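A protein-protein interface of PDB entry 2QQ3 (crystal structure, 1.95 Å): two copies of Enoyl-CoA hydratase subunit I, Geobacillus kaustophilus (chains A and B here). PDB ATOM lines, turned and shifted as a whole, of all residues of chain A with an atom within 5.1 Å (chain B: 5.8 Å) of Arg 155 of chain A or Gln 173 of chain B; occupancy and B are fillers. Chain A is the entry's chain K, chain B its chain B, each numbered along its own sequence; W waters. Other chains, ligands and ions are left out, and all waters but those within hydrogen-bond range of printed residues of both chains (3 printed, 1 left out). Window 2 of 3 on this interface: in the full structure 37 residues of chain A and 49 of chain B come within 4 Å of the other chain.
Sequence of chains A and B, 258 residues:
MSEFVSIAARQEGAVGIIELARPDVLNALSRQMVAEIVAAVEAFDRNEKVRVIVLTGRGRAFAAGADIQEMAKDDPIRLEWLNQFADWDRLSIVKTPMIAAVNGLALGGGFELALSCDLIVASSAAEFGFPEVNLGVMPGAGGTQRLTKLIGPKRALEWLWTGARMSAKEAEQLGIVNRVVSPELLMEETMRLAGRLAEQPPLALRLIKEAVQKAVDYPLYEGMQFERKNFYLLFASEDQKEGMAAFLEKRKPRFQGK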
ATOM      1  N   ILE A 151     -26.540  -1.660  11.293  1.00  0.00           N
ATOM      2  CA  ILE A 151     -25.906  -1.323  12.569  1.00  0.00           C
ATOM      3  C   ILE A 151     -24.403  -1.045  12.576  1.00  0.00           C
ATOM      4  O   ILE A 151     -23.811  -0.874  13.644  1.00  0.00           O
ATOM      5  CB  ILE A 151     -26.177  -2.425  13.610  1.00  0.00           C
ATOM      6  CG1 ILE A 151     -25.442  -3.708  13.215  1.00  0.00           C
ATOM      7  CG2 ILE A 151     -27.671  -2.676  13.715  1.00  0.00           C
ATOM      8  CD1 ILE A 151     -25.632  -4.855  14.207  1.00  0.00           C
ATOM      9  N   GLY A 152     -23.778  -1.005  11.406  1.00  0.00           N
ATOM     10  CA  GLY A 152     -22.349  -0.737  11.359  1.00  0.00           C
ATOM     11  C   GLY A 152     -21.482  -1.976  11.507  1.00  0.00           C
ATOM     12  O   GLY A 152     -21.906  -2.969  12.094  1.00  0.00           O
ATOM     13  N   PRO A 153     -20.244  -1.937  10.993  1.00  0.00           N
ATOM     14  CA  PRO A 153     -19.294  -3.051  11.049  1.00  0.00           C
ATOM     15  C   PRO A 153     -18.854  -3.511  12.439  1.00  0.00           C
ATOM     16  O   PRO A 153     -18.714  -4.710  12.675  1.00  0.00           O
ATOM     17  CB  PRO A 153     -18.124  -2.549  10.201  1.00  0.00           C
ATOM     18  CG  PRO A 153     -18.186  -1.052  10.388  1.00  0.00           C
ATOM     19  CD  PRO A 153     -19.660  -0.784  10.282  1.00  0.00           C
ATOM     20  N   LYS A 154     -18.617  -2.564  13.345  1.00  0.00           N
ATOM     21  CA  LYS A 154     -18.185  -2.905  14.701  1.00  0.00           C
ATOM     22  C   LYS A 154     -19.214  -3.824  15.367  1.00  0.00           C
ATOM     23  O   LYS A 154     -18.885  -4.926  15.812  1.00  0.00           O
ATOM     24  CB  LYS A 154     -17.987  -1.630  15.532  1.00  0.00           C
ATOM     25  CG  LYS A 154     -16.821  -0.736  15.063  1.00  0.00           C
ATOM     26  CD  LYS A 154     -15.473  -1.290  15.524  1.00  0.00           C
ATOM     27  CE  LYS A 154     -14.295  -0.403  15.098  1.00  0.00           C
ATOM     28  NZ  LYS A 154     -14.054  -0.430  13.622  1.00  0.00           N
ATOM     29  N   ARG A 155     -20.464  -3.376  15.429  1.00  0.00           N
ATOM     30  CA  ARG A 155     -21.511  -4.187  16.033  1.00  0.00           C
ATOM     31  C   ARG A 155     -21.849  -5.413  15.178  1.00  0.00           C
ATOM     32  O   ARG A 155     -22.060  -6.504  15.708  1.00  0.00           O
ATOM     33  CB  ARG A 155     -22.759  -3.331  16.283  1.00  0.00           C
ATOM     34  CG  ARG A 155     -22.531  -2.248  17.351  1.00  0.00           C
ATOM     35  CD  ARG A 155     -23.777  -1.424  17.659  1.00  0.00           C
ATOM     36  NE  ARG A 155     -24.159  -0.577  16.537  1.00  0.00           N
ATOM     37  CZ  ARG A 155     -24.895   0.528  16.641  1.00  0.00           C
ATOM     38  NH1 ARG A 155     -25.339   0.935  17.828  1.00  0.00           N
ATOM     39  NH2 ARG A 155     -25.180   1.231  15.550  1.00  0.00           N
ATOM     40  N   ALA A 156     -21.878  -5.248  13.858  1.00  0.00           N
ATOM     41  CA  ALA A 156     -22.195  -6.368  12.970  1.00  0.00           C
ATOM     42  C   ALA A 156     -21.246  -7.551  13.173  1.00  0.00           C
ATOM     43  O   ALA A 156     -21.689  -8.693  13.311  1.00  0.00           O
ATOM     44  CB  ALA A 156     -22.150  -5.917  11.514  1.00  0.00           C
ATOM     45  N   LEU A 157     -19.946  -7.275  13.181  1.00  0.00           N
ATOM     46  CA  LEU A 157     -18.941  -8.322  13.354  1.00  0.00           C
ATOM     47  C   LEU A 157     -19.070  -9.050  14.681  1.00  0.00           C
ATOM     48  O   LEU A 157     -18.834 -10.253  14.754  1.00  0.00           O
ATOM     49  CB  LEU A 157     -17.531  -7.740  13.235  1.00  0.00           C
ATOM     50  CG  LEU A 157     -16.985  -7.581  11.815  1.00  0.00           C
ATOM     51  CD1 LEU A 157     -15.632  -6.894  11.866  1.00  0.00           C
ATOM     52  CD2 LEU A 157     -16.867  -8.957  11.155  1.00  0.00           C
ATOM     53  N   GLU A 158     -19.438  -8.323  15.731  1.00  0.00           N
ATOM     54  CA  GLU A 158     -19.598  -8.941  17.039  1.00  0.00           C
ATOM     55  C   GLU A 158     -20.671 -10.031  16.985  1.00  0.00           C
ATOM     56  O   GLU A 158     -20.466 -11.139  17.482  1.00  0.00           O
ATOM     57  CB  GLU A 158     -19.990  -7.895  18.079  1.00  0.00           C
ATOM     58  CG  GLU A 158     -19.772  -8.356  19.508  1.00  0.00           C
ATOM     59  CD  GLU A 158     -20.392  -7.421  20.526  1.00  0.00           C
ATOM     60  OE1 GLU A 158     -20.345  -6.190  20.322  1.00  0.00           O
ATOM     61  OE2 GLU A 158     -20.920  -7.924  21.539  1.00  0.00           O
ATOM     62  N   TRP A 159     -21.812  -9.716  16.378  1.00  0.00           N
ATOM     63  CA  TRP A 159     -22.903 -10.676  16.273  1.00  0.00           C
ATOM     64  C   TRP A 159     -22.596 -11.797  15.284  1.00  0.00           C
ATOM     65  O   TRP A 159     -22.881 -12.967  15.551  1.00  0.00           O
ATOM     66  CB  TRP A 159     -24.209  -9.977  15.864  1.00  0.00           C
ATOM     67  CG  TRP A 159     -24.750  -9.070  16.930  1.00  0.00           C
ATOM     68  CD1 TRP A 159     -24.637  -7.708  16.993  1.00  0.00           C
ATOM     69  CD2 TRP A 159     -25.410  -9.472  18.136  1.00  0.00           C
ATOM     70  NE1 TRP A 159     -25.180  -7.241  18.168  1.00  0.00           N
ATOM     71  CE2 TRP A 159     -25.660  -8.303  18.886  1.00  0.00           C
ATOM     72  CE3 TRP A 159     -25.809 -10.712  18.656  1.00  0.00           C
ATOM     73  CZ2 TRP A 159     -26.294  -8.335  20.134  1.00  0.00           C
ATOM     74  CZ3 TRP A 159     -26.440 -10.746  19.899  1.00  0.00           C
ATOM     75  CH2 TRP A 159     -26.675  -9.563  20.622  1.00  0.00           C
ATOM     76  N   LEU A 174     -31.492  -0.815  17.921  1.00  0.00           N
ATOM     77  CA  LEU A 174     -30.533  -0.718  16.821  1.00  0.00           C
ATOM     78  C   LEU A 174     -31.142  -0.285  15.484  1.00  0.00           C
ATOM     79  O   LEU A 174     -30.415  -0.043  14.516  1.00  0.00           O
ATOM     80  CB  LEU A 174     -29.814  -2.059  16.637  1.00  0.00           C
ATOM     81  CG  LEU A 174     -28.817  -2.436  17.736  1.00  0.00           C
ATOM     82  CD1 LEU A 174     -28.375  -3.880  17.556  1.00  0.00           C
ATOM     83  CD2 LEU A 174     -27.622  -1.491  17.695  1.00  0.00           C
ATOM     84  N   LEU B 150     -19.748   5.198  10.723  1.00  0.00           N
ATOM     85  CA  LEU B 150     -20.300   4.641  11.951  1.00  0.00           C
ATOM     86  C   LEU B 150     -21.447   5.449  12.549  1.00  0.00           C
ATOM     87  O   LEU B 150     -22.458   4.882  12.951  1.00  0.00           O
ATOM     88  CB  LEU B 150     -19.194   4.487  13.004  1.00  0.00           C
ATOM     89  CG  LEU B 150     -18.195   3.347  12.755  1.00  0.00           C
ATOM     90  CD1 LEU B 150     -16.992   3.466  13.693  1.00  0.00           C
ATOM     91  CD2 LEU B 150     -18.909   2.025  12.959  1.00  0.00           C
ATOM     92  N   ALA B 168     -16.349   6.872  26.730  1.00  0.00           N
ATOM     93  CA  ALA B 168     -16.429   5.483  26.310  1.00  0.00           C
ATOM     94  C   ALA B 168     -17.897   5.065  26.254  1.00  0.00           C
ATOM     95  O   ALA B 168     -18.309   4.327  25.360  1.00  0.00           O
ATOM     96  CB  ALA B 168     -15.660   4.589  27.281  1.00  0.00           C
ATOM     97  N   LYS B 169     -18.683   5.549  27.211  1.00  0.00           N
ATOM     98  CA  LYS B 169     -20.104   5.228  27.269  1.00  0.00           C
ATOM     99  C   LYS B 169     -20.840   5.699  26.013  1.00  0.00           C
ATOM    100  O   LYS B 169     -21.667   4.975  25.469  1.00  0.00           O
ATOM    101  CB  LYS B 169     -20.748   5.873  28.504  1.00  0.00           C
ATOM    102  CG  LYS B 169     -22.262   5.703  28.588  1.00  0.00           C
ATOM    103  CD  LYS B 169     -22.657   4.320  29.086  1.00  0.00           C
ATOM    104  CE  LYS B 169     -22.310   4.145  30.561  1.00  0.00           C
ATOM    105  NZ  LYS B 169     -22.742   2.823  31.102  1.00  0.00           N
ATOM    106  N   GLU B 170     -20.554   6.916  25.559  1.00  0.00           N
ATOM    107  CA  GLU B 170     -21.222   7.420  24.364  1.00  0.00           C
ATOM    108  C   GLU B 170     -20.740   6.686  23.114  1.00  0.00           C
ATOM    109  O   GLU B 170     -21.516   6.436  22.187  1.00  0.00           O
ATOM    110  CB  GLU B 170     -21.003   8.930  24.208  1.00  0.00           C
ATOM    111  CG  GLU B 170     -21.518   9.472  22.872  1.00  0.00           C
ATOM    112  CD  GLU B 170     -21.907  10.941  22.916  1.00  0.00           C
ATOM    113  OE1 GLU B 170     -21.219  11.732  23.597  1.00  0.00           O
ATOM    114  OE2 GLU B 170     -22.899  11.302  22.247  1.00  0.00           O
ATOM    115  N   ALA B 171     -19.460   6.334  23.091  1.00  0.00           N
ATOM    116  CA  ALA B 171     -18.895   5.620  21.953  1.00  0.00           C
ATOM    117  C   ALA B 171     -19.606   4.275  21.810  1.00  0.00           C
ATOM    118  O   ALA B 171     -19.885   3.814  20.702  1.00  0.00           O
ATOM    119  CB  ALA B 171     -17.397   5.407  22.160  1.00  0.00           C
ATOM    120  N   GLU B 172     -19.910   3.652  22.944  1.00  0.00           N
ATOM    121  CA  GLU B 172     -20.588   2.368  22.939  1.00  0.00           C
ATOM    122  C   GLU B 172     -22.030   2.515  22.442  1.00  0.00           C
ATOM    123  O   GLU B 172     -22.501   1.706  21.646  1.00  0.00           O
ATOM    124  CB  GLU B 172     -20.553   1.763  24.348  1.00  0.00           C
ATOM    125  CG  GLU B 172     -21.069   0.331  24.460  1.00  0.00           C
ATOM    126  CD  GLU B 172     -22.570   0.226  24.268  1.00  0.00           C
ATOM    127  OE1 GLU B 172     -23.305   1.026  24.885  1.00  0.00           O
ATOM    128  OE2 GLU B 172     -23.019  -0.662  23.511  1.00  0.00           O
ATOM    129  N   GLN B 173     -22.724   3.557  22.887  1.00  0.00           N
ATOM    130  CA  GLN B 173     -24.109   3.760  22.469  1.00  0.00           C
ATOM    131  C   GLN B 173     -24.196   4.074  20.977  1.00  0.00           C
ATOM    132  O   GLN B 173     -25.165   3.710  20.316  1.00  0.00           O
ATOM    133  CB  GLN B 173     -24.754   4.899  23.271  1.00  0.00           C
ATOM    134  CG  GLN B 173     -24.327   4.946  24.732  1.00  0.00           C
ATOM    135  CD  GLN B 173     -24.455   3.604  25.437  1.00  0.00           C
ATOM    136  OE1 GLN B 173     -23.747   3.332  26.411  1.00  0.00           O
ATOM    137  NE2 GLN B 173     -25.366   2.761  24.955  1.00  0.00           N
ATOM    138  N   LEU B 174     -23.174   4.745  20.455  1.00  0.00           N
ATOM    139  CA  LEU B 174     -23.130   5.114  19.045  1.00  0.00           C
ATOM    140  C   LEU B 174     -22.737   3.954  18.130  1.00  0.00           C
ATOM    141  O   LEU B 174     -22.876   4.049  16.910  1.00  0.00           O
ATOM    142  CB  LEU B 174     -22.155   6.278  18.836  1.00  0.00           C
ATOM    143  CG  LEU B 174     -22.523   7.629  19.460  1.00  0.00           C
ATOM    144  CD1 LEU B 174     -21.396   8.626  19.221  1.00  0.00           C
ATOM    145  CD2 LEU B 174     -23.822   8.141  18.859  1.00  0.00           C
ATOM    146  N   GLY B 175     -22.239   2.867  18.715  1.00  0.00           N
ATOM    147  CA  GLY B 175     -21.851   1.716  17.918  1.00  0.00           C
ATOM    148  C   GLY B 175     -20.398   1.732  17.475  1.00  0.00           C
ATOM    149  O   GLY B 175     -20.015   0.996  16.560  1.00  0.00           O
ATOM    150  N   ILE B 176     -19.594   2.574  18.118  1.00  0.00           N
ATOM    151  CA  ILE B 176     -18.173   2.689  17.816  1.00  0.00           C
ATOM    152  C   ILE B 176     -17.400   1.676  18.664  1.00  0.00           C
ATOM    153  O   ILE B 176     -16.486   0.997  18.179  1.00  0.00           O
ATOM    154  CB  ILE B 176     -17.658   4.118  18.137  1.00  0.00           C
ATOM    155  CG1 ILE B 176     -18.391   5.141  17.262  1.00  0.00           C
ATOM    156  CG2 ILE B 176     -16.149   4.204  17.899  1.00  0.00           C
ATOM    157  CD1 ILE B 176     -18.074   6.588  17.605  1.00  0.00           C
ATOM    158  N   VAL B 177     -17.783   1.585  19.934  1.00  0.00           N
ATOM    159  CA  VAL B 177     -17.164   0.670  20.890  1.00  0.00           C
ATOM    160  C   VAL B 177     -18.103  -0.516  21.133  1.00  0.00           C
ATOM    161  O   VAL B 177     -19.319  -0.343  21.229  1.00  0.00           O
ATOM    162  CB  VAL B 177     -16.858   1.415  22.228  1.00  0.00           C
ATOM    163  CG1 VAL B 177     -16.686   0.436  23.372  1.00  0.00           C
ATOM    164  CG2 VAL B 177     -15.583   2.240  22.071  1.00  0.00           C
ATOM    165  N   ASN B 178     -17.539  -1.717  21.228  1.00  0.00           N
ATOM    166  CA  ASN B 178     -18.331  -2.930  21.440  1.00  0.00           C
ATOM    167  C   ASN B 178     -18.681  -3.198  22.897  1.00  0.00           C
ATOM    168  O   ASN B 178     -19.782  -3.659  23.204  1.00  0.00           O
ATOM    169  CB  ASN B 178     -17.584  -4.149  20.898  1.00  0.00           C
ATOM    170  CG  ASN B 178     -17.449  -4.122  19.400  1.00  0.00           C
ATOM    171  OD1 ASN B 178     -18.348  -4.548  18.679  1.00  0.00           O
ATOM    172  ND2 ASN B 178     -16.331  -3.599  18.922  1.00  0.00           N
HETATM  173  O   HOH W   1     -26.707   4.069  17.733  1.00  0.00           O
HETATM  174  O   HOH W   2     -25.006   0.200  20.342  1.00  0.00           O
HETATM  175  O   HOH W   3     -22.509  -3.792  21.168  1.00  0.00           O
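The backbone carbonyl oxygen (O) of Lys 154 of chain A sits close to the side-chain amide oxygen (OD1) of Asn 178 of chain B (2.9 Å).
The side-chain amide oxygen (OD1) of Asn 178 of chain B lies close to the side-chain carboxylate (OE1) of Glu 158 of chain A (3.1 Å).
O of Lys 169 of chain B sits close to OE1 of Gln 173 of chain B (2.8 Å).
The backbone NH of Ile 176 of chain B sits at hydrogen-bond distance from the backbone carbonyl oxygen of Ala 171 of chain B, at 2.9 Å.
The side-chain amide nitrogen (NE2) of Gln 173 of chain B sits at hydrogen-bond distance from the side-chain carboxylate (OE1) of Glu 172 of chain B (2.7 Å).
O of Ile 151 of chain A lies within hydrogen-bond range of NE of Arg 155 of chain A.
Among the printed residues, merely in contact across the chains: Lys 154 of chain A with Gly 175 of chain B (3.5 Å), Arg 155 of chain A with Gly 175 of chain B (3.5 Å), Lys 154 of chain A with Ile 176 of chain B (3.6 Å), Arg 155 of chain A with Gln 173 of chain B (3.7 Å), Arg 155 of chain A with Leu 174 of chain B (3.9 Å) and Pro 153 of chain A with Leu 150 of chain B (3.95 Å).
Arg 155 of chain A touches just these residues of chain B: Gln 173, Leu 174 and Gly 175.
Gln 173 of chain B touches just one residue of chain A: Arg 155.
Printed residues of chain A within 4 Å of Asn 178 of chain B: Lys 154 and Glu 158.
Of the printed residues of chain B, Glu 158 of chain A touches Asn 178.
Printed residues of chain A within 4 Å of Gly 175 of chain B: Lys 154 (3.5 Å) and Arg 155 (3.5 Å).
Of the printed residues of chain A, Leu 174 of chain B touches Arg 155 (3.9 Å).
Of the printed residues of chain B, Pro 153 of chain A touches Leu 150.
The nearest printed residue of chain A that does not touch Gln 173 of chain B is Leu 174 of chain A (6.3 Å).
Of the 12 printed residues of chain B, 6 touch a printed residue of chain A.
Hydrophobic or aromatic side chains of chain B that line the printed part of chain A: Leu 150.
Of the 10 printed residues of chain A, 4 touch a printed residue of chain B.
1 position is printed for both chains.
Water W2 bridges the guanidinium group (NH1) of Arg 155 of chain A and the backbone carbonyl oxygen (O) of Glu 172 of chain B.
Water W1 lies within hydrogen-bond range of the backbone carbonyl oxygen (O) of Gln 173 of chain B (3.0 Å) and the guanidinium group (NH1) of Arg 155 of chain A (3.4 Å).
Water W3 bridges OE1 of Glu 158 of chain A (3.3 Å) and O of Asn 178 of chain B (3.4 Å).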
